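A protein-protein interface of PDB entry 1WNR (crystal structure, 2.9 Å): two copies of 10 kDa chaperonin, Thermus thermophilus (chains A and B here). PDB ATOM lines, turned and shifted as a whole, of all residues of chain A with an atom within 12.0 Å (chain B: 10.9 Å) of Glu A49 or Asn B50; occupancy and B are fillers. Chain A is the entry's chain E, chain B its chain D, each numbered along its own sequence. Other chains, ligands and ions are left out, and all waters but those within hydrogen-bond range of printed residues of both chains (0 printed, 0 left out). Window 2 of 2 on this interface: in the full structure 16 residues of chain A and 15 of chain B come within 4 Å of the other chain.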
ATOM      1  N   GLY A  45      19.430   5.096  10.447  1.00  0.00           N
ATOM      2  CA  GLY A  45      18.802   4.575   9.249  1.00  0.00           C
ATOM      3  C   GLY A  45      17.323   4.293   9.360  1.00  0.00           C
ATOM      4  O   GLY A  45      16.753   4.278  10.444  1.00  0.00           O
ATOM      5  N   ARG A  46      16.714   4.062   8.206  1.00  0.00           N
ATOM      6  CA  ARG A  46      15.292   3.774   8.073  1.00  0.00           C
ATOM      7  C   ARG A  46      14.912   2.387   8.582  1.00  0.00           C
ATOM      8  O   ARG A  46      15.684   1.444   8.446  1.00  0.00           O
ATOM      9  CB  ARG A  46      14.926   3.907   6.600  1.00  0.00           C
ATOM     10  CG  ARG A  46      13.768   3.071   6.160  1.00  0.00           C
ATOM     11  CD  ARG A  46      13.675   3.068   4.647  1.00  0.00           C
ATOM     12  NE  ARG A  46      14.985   2.856   4.035  1.00  0.00           N
ATOM     13  CZ  ARG A  46      15.162   2.391   2.803  1.00  0.00           C
ATOM     14  NH1 ARG A  46      14.101   2.082   2.056  1.00  0.00           N
ATOM     15  NH2 ARG A  46      16.395   2.239   2.318  1.00  0.00           N
ATOM     16  N   VAL A  47      13.725   2.267   9.176  1.00  0.00           N
ATOM     17  CA  VAL A  47      13.250   0.973   9.673  1.00  0.00           C
ATOM     18  C   VAL A  47      12.216   0.418   8.704  1.00  0.00           C
ATOM     19  O   VAL A  47      11.283   1.117   8.327  1.00  0.00           O
ATOM     20  CB  VAL A  47      12.563   1.082  11.038  1.00  0.00           C
ATOM     21  CG1 VAL A  47      12.148  -0.298  11.505  1.00  0.00           C
ATOM     22  CG2 VAL A  47      13.485   1.721  12.042  1.00  0.00           C
ATOM     23  N   LEU A  48      12.380  -0.840   8.315  1.00  0.00           N
ATOM     24  CA  LEU A  48      11.466  -1.485   7.378  1.00  0.00           C
ATOM     25  C   LEU A  48      10.313  -2.207   8.071  1.00  0.00           C
ATOM     26  O   LEU A  48      10.433  -2.645   9.214  1.00  0.00           O
ATOM     27  CB  LEU A  48      12.218  -2.493   6.516  1.00  0.00           C
ATOM     28  CG  LEU A  48      13.492  -1.997   5.856  1.00  0.00           C
ATOM     29  CD1 LEU A  48      14.016  -3.094   4.955  1.00  0.00           C
ATOM     30  CD2 LEU A  48      13.213  -0.731   5.073  1.00  0.00           C
ATOM     31  N   GLU A  49       9.206  -2.355   7.354  1.00  0.00           N
ATOM     32  CA  GLU A  49       8.029  -3.009   7.903  1.00  0.00           C
ATOM     33  C   GLU A  49       8.286  -4.421   8.422  1.00  0.00           C
ATOM     34  O   GLU A  49       7.478  -4.959   9.186  1.00  0.00           O
ATOM     35  CB  GLU A  49       6.906  -3.018   6.863  1.00  0.00           C
ATOM     36  CG  GLU A  49       6.361  -1.630   6.535  1.00  0.00           C
ATOM     37  CD  GLU A  49       5.781  -0.922   7.751  1.00  0.00           C
ATOM     38  OE1 GLU A  49       4.851  -1.477   8.379  1.00  0.00           O
ATOM     39  OE2 GLU A  49       6.256   0.190   8.081  1.00  0.00           O
ATOM     40  N   ASN A  50       9.404  -5.021   8.020  1.00  0.00           N
ATOM     41  CA  ASN A  50       9.740  -6.366   8.477  1.00  0.00           C
ATOM     42  C   ASN A  50      10.607  -6.262   9.726  1.00  0.00           C
ATOM     43  O   ASN A  50      11.130  -7.257  10.226  1.00  0.00           O
ATOM     44  CB  ASN A  50      10.478  -7.142   7.381  1.00  0.00           C
ATOM     45  CG  ASN A  50      11.945  -6.777   7.289  1.00  0.00           C
ATOM     46  OD1 ASN A  50      12.323  -5.615   7.452  1.00  0.00           O
ATOM     47  ND2 ASN A  50      12.782  -7.769   7.012  1.00  0.00           N
ATOM     48  N   GLY A  51      10.755  -5.038  10.220  1.00  0.00           N
ATOM     49  CA  GLY A  51      11.542  -4.811  11.415  1.00  0.00           C
ATOM     50  C   GLY A  51      12.995  -4.448  11.181  1.00  0.00           C
ATOM     51  O   GLY A  51      13.598  -3.770  12.011  1.00  0.00           O
ATOM     52  N   GLN A  52      13.562  -4.891  10.062  1.00  0.00           N
ATOM     53  CA  GLN A  52      14.965  -4.607   9.753  1.00  0.00           C
ATOM     54  C   GLN A  52      15.286  -3.125   9.659  1.00  0.00           C
ATOM     55  O   GLN A  52      14.427  -2.313   9.316  1.00  0.00           O
ATOM     56  CB  GLN A  52      15.366  -5.279   8.438  1.00  0.00           C
ATOM     57  CG  GLN A  52      15.588  -6.779   8.539  1.00  0.00           C
ATOM     58  CD  GLN A  52      15.980  -7.410   7.213  1.00  0.00           C
ATOM     59  OE1 GLN A  52      16.210  -8.617   7.134  1.00  0.00           O
ATOM     60  NE2 GLN A  52      16.057  -6.596   6.165  1.00  0.00           N
ATOM     61  N   ARG A  53      16.532  -2.776   9.962  1.00  0.00           N
ATOM     62  CA  ARG A  53      16.966  -1.383   9.896  1.00  0.00           C
ATOM     63  C   ARG A  53      18.018  -1.240   8.795  1.00  0.00           C
ATOM     64  O   ARG A  53      19.049  -1.910   8.830  1.00  0.00           O
ATOM     65  CB  ARG A  53      17.547  -0.954  11.244  1.00  0.00           C
ATOM     66  CG  ARG A  53      17.735   0.546  11.411  1.00  0.00           C
ATOM     67  CD  ARG A  53      18.267   0.874  12.808  1.00  0.00           C
ATOM     68  NE  ARG A  53      17.293   0.602  13.868  1.00  0.00           N
ATOM     69  CZ  ARG A  53      16.312   1.429  14.227  1.00  0.00           C
ATOM     70  NH1 ARG A  53      16.162   2.602  13.614  1.00  0.00           N
ATOM     71  NH2 ARG A  53      15.478   1.079  15.199  1.00  0.00           N
ATOM     72  N   VAL A  54      17.754  -0.385   7.810  1.00  0.00           N
ATOM     73  CA  VAL A  54      18.690  -0.175   6.706  1.00  0.00           C
ATOM     74  C   VAL A  54      19.670   0.936   7.046  1.00  0.00           C
ATOM     75  O   VAL A  54      19.277   2.085   7.271  1.00  0.00           O
ATOM     76  CB  VAL A  54      17.951   0.212   5.417  1.00  0.00           C
ATOM     77  CG1 VAL A  54      18.925   0.331   4.260  1.00  0.00           C
ATOM     78  CG2 VAL A  54      16.898  -0.821   5.119  1.00  0.00           C
ATOM     79  N   ASP B   7       3.374   6.447  18.231  1.00  0.00           N
ATOM     80  CA  ASP B   7       4.662   6.965  17.816  1.00  0.00           C
ATOM     81  C   ASP B   7       4.793   8.458  18.114  1.00  0.00           C
ATOM     82  O   ASP B   7       5.218   9.235  17.253  1.00  0.00           O
ATOM     83  CB  ASP B   7       4.783   6.707  16.319  1.00  0.00           C
ATOM     84  CG  ASP B   7       6.118   7.083  15.777  1.00  0.00           C
ATOM     85  OD1 ASP B   7       7.119   6.483  16.247  1.00  0.00           O
ATOM     86  OD2 ASP B   7       6.152   7.972  14.889  1.00  0.00           O
ATOM     87  N   GLY B  45       5.674   4.026  20.624  1.00  0.00           N
ATOM     88  CA  GLY B  45       6.232   3.884  19.297  1.00  0.00           C
ATOM     89  C   GLY B  45       5.297   3.339  18.242  1.00  0.00           C
ATOM     90  O   GLY B  45       4.151   2.969  18.516  1.00  0.00           O
ATOM     91  N   ARG B  46       5.821   3.292  17.023  1.00  0.00           N
ATOM     92  CA  ARG B  46       5.109   2.806  15.857  1.00  0.00           C
ATOM     93  C   ARG B  46       4.959   1.280  15.809  1.00  0.00           C
ATOM     94  O   ARG B  46       5.818   0.539  16.292  1.00  0.00           O
ATOM     95  CB  ARG B  46       5.836   3.290  14.600  1.00  0.00           C
ATOM     96  CG  ARG B  46       5.586   2.441  13.371  1.00  0.00           C
ATOM     97  CD  ARG B  46       6.566   2.753  12.252  1.00  0.00           C
ATOM     98  NE  ARG B  46       7.920   2.954  12.758  1.00  0.00           N
ATOM     99  CZ  ARG B  46       9.010   2.940  11.996  1.00  0.00           C
ATOM    100  NH1 ARG B  46       8.895   2.720  10.684  1.00  0.00           N
ATOM    101  NH2 ARG B  46      10.209   3.167  12.542  1.00  0.00           N
ATOM    102  N   VAL B  47       3.853   0.826  15.223  1.00  0.00           N
ATOM    103  CA  VAL B  47       3.578  -0.597  15.057  1.00  0.00           C
ATOM    104  C   VAL B  47       3.826  -0.908  13.585  1.00  0.00           C
ATOM    105  O   VAL B  47       3.390  -0.166  12.714  1.00  0.00           O
ATOM    106  CB  VAL B  47       2.111  -0.944  15.371  1.00  0.00           C
ATOM    107  CG1 VAL B  47       1.921  -2.459  15.363  1.00  0.00           C
ATOM    108  CG2 VAL B  47       1.718  -0.362  16.696  1.00  0.00           C
ATOM    109  N   LEU B  48       4.537  -1.993  13.311  1.00  0.00           N
ATOM    110  CA  LEU B  48       4.826  -2.377  11.937  1.00  0.00           C
ATOM    111  C   LEU B  48       3.786  -3.402  11.476  1.00  0.00           C
ATOM    112  O   LEU B  48       3.005  -3.913  12.288  1.00  0.00           O
ATOM    113  CB  LEU B  48       6.234  -2.974  11.852  1.00  0.00           C
ATOM    114  CG  LEU B  48       7.397  -2.123  12.360  1.00  0.00           C
ATOM    115  CD1 LEU B  48       8.683  -2.902  12.201  1.00  0.00           C
ATOM    116  CD2 LEU B  48       7.467  -0.820  11.589  1.00  0.00           C
ATOM    117  N   GLU B  49       3.777  -3.707  10.180  1.00  0.00           N
ATOM    118  CA  GLU B  49       2.826  -4.675   9.636  1.00  0.00           C
ATOM    119  C   GLU B  49       3.029  -6.097  10.151  1.00  0.00           C
ATOM    120  O   GLU B  49       2.128  -6.924  10.066  1.00  0.00           O
ATOM    121  CB  GLU B  49       2.884  -4.678   8.105  1.00  0.00           C
ATOM    122  CG  GLU B  49       2.273  -3.436   7.473  1.00  0.00           C
ATOM    123  CD  GLU B  49       0.826  -3.212   7.923  1.00  0.00           C
ATOM    124  OE1 GLU B  49      -0.034  -4.088   7.647  1.00  0.00           O
ATOM    125  OE2 GLU B  49       0.550  -2.163   8.559  1.00  0.00           O
ATOM    126  N   ASN B  50       4.207  -6.389  10.687  1.00  0.00           N
ATOM    127  CA  ASN B  50       4.470  -7.726  11.180  1.00  0.00           C
ATOM    128  C   ASN B  50       4.053  -7.780  12.625  1.00  0.00           C
ATOM    129  O   ASN B  50       4.251  -8.779  13.304  1.00  0.00           O
ATOM    130  CB  ASN B  50       5.953  -8.051  11.043  1.00  0.00           C
ATOM    131  CG  ASN B  50       6.806  -7.301  12.044  1.00  0.00           C
ATOM    132  OD1 ASN B  50       6.585  -6.112  12.302  1.00  0.00           O
ATOM    133  ND2 ASN B  50       7.796  -7.991  12.610  1.00  0.00           N
ATOM    134  N   GLY B  51       3.477  -6.683  13.094  1.00  0.00           N
ATOM    135  CA  GLY B  51       3.018  -6.628  14.466  1.00  0.00           C
ATOM    136  C   GLY B  51       4.010  -6.031  15.444  1.00  0.00           C
ATOM    137  O   GLY B  51       3.614  -5.517  16.492  1.00  0.00           O
ATOM    138  N   GLN B  52       5.298  -6.095  15.117  1.00  0.00           N
ATOM    139  CA  GLN B  52       6.324  -5.551  16.002  1.00  0.00           C
ATOM    140  C   GLN B  52       6.107  -4.068  16.276  1.00  0.00           C
ATOM    141  O   GLN B  52       5.566  -3.335  15.449  1.00  0.00           O
ATOM    142  CB  GLN B  52       7.721  -5.747  15.407  1.00  0.00           C
ATOM    143  CG  GLN B  52       8.192  -7.183  15.336  1.00  0.00           C
ATOM    144  CD  GLN B  52       9.548  -7.305  14.653  1.00  0.00           C
ATOM    145  OE1 GLN B  52       9.962  -8.400  14.267  1.00  0.00           O
ATOM    146  NE2 GLN B  52      10.245  -6.180  14.502  1.00  0.00           N
ATOM    147  N   ARG B  53       6.557  -3.636  17.446  1.00  0.00           N
ATOM    148  CA  ARG B  53       6.423  -2.248  17.854  1.00  0.00           C
ATOM    149  C   ARG B  53       7.792  -1.594  17.990  1.00  0.00           C
ATOM    150  O   ARG B  53       8.550  -1.898  18.903  1.00  0.00           O
ATOM    151  CB  ARG B  53       5.671  -2.183  19.184  1.00  0.00           C
ATOM    152  CG  ARG B  53       5.344  -0.788  19.667  1.00  0.00           C
ATOM    153  CD  ARG B  53       4.605  -0.854  20.989  1.00  0.00           C
ATOM    154  NE  ARG B  53       3.292  -1.461  20.823  1.00  0.00           N
ATOM    155  CZ  ARG B  53       2.246  -0.834  20.295  1.00  0.00           C
ATOM    156  NH1 ARG B  53       2.370   0.426  19.891  1.00  0.00           N
ATOM    157  NH2 ARG B  53       1.079  -1.463  20.163  1.00  0.00           N
ATOM    158  N   VAL B  54       8.104  -0.694  17.068  1.00  0.00           N
ATOM    159  CA  VAL B  54       9.378   0.006  17.089  1.00  0.00           C
ATOM    160  C   VAL B  54       9.373   1.067  18.184  1.00  0.00           C
ATOM    161  O   VAL B  54       8.516   1.954  18.196  1.00  0.00           O
ATOM    162  CB  VAL B  54       9.646   0.707  15.759  1.00  0.00           C
ATOM    163  CG1 VAL B  54      11.046   1.274  15.757  1.00  0.00           C
ATOM    164  CG2 VAL B  54       9.451  -0.259  14.614  1.00  0.00           C
ATOM    165  N   PRO B  55      10.340   0.991  19.114  1.00  0.00           N
ATOM    166  CA  PRO B  55      10.468   1.935  20.232  1.00  0.00           C
ATOM    167  C   PRO B  55      10.967   3.284  19.749  1.00  0.00           C
ATOM    168  O   PRO B  55      11.759   3.352  18.803  1.00  0.00           O
ATOM    169  CB  PRO B  55      11.498   1.271  21.140  1.00  0.00           C
ATOM    170  CG  PRO B  55      11.495  -0.160  20.709  1.00  0.00           C
ATOM    171  CD  PRO B  55      11.347  -0.072  19.227  1.00  0.00           C
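The side-chain amide nitrogen of Asn B50 lies within hydrogen-bond range of the side-chain amide oxygen of Gln B52, 2.8 Å away. The backbone carbonyl oxygen (O) of Arg B46 is in hydrogen-bond range of the backbone NH (N) of Val B54 (2.7 Å).
Of the 10 printed residues of chain A, 4 touch a printed residue of chain B. Printed residues of chain B that touch a printed residue of chain A: Arg B46, Leu B48, Glu B49, Asn B50 and Gln B52. Among the printed residues, 7 pairs touch across the chains. Among the printed residues, no Asp or Glu carboxylate lies within 4 Å of a Lys or Arg side-chain nitrogen of the other chain.
Printed residues of chain B within 4 Å of Val A47: Arg B46. Glu A49 touches three residues of chain B. No residue of chain B comes within 4 Å of Asn A50. Of the printed residues of chain A, Arg B46 touches Val A47 (3.5 Å). Of the printed residues of chain A, Leu B48 touches Leu A48, Glu A49 and Gly A51. Asn B50 touches just one residue of chain A: Glu A49. Gly B51 touches none of the printed residues of chain A. Arg B53 touches none of the printed residues of chain A. The nearest residue of chain A that does not touch Asn B50 is Asn A50 (4.2 Å).
Arg B46 touches Val A47. Leu B48 touches Leu A48. Glu A49 touches Leu B48. Gly A51 touches Leu B48 (CA to CD1, 3.5 Å). Gln B52 touches Gly A51.
Glu A49 touches Leu B48, but with the chains exchanged Leu A48 does not touch Glu B49 (6.8 Å). Glu A49 touches its own counterpart, Glu B49. Glu A49 touches Asn B50, but with the chains exchanged Asn A50 does not touch Glu B49 (6.2 Å). Gly A51 touches Leu B48, but with the chains exchanged Leu A48 does not touch Gly B51 (8.9 Å).
N of Glu B49 lies within hydrogen-bond range of OE1 of Glu A49. The side-chain amide oxygen (OD1) of Asn B50 lies close to the backbone carbonyl oxygen (O) of Glu A49 (3.4 Å).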
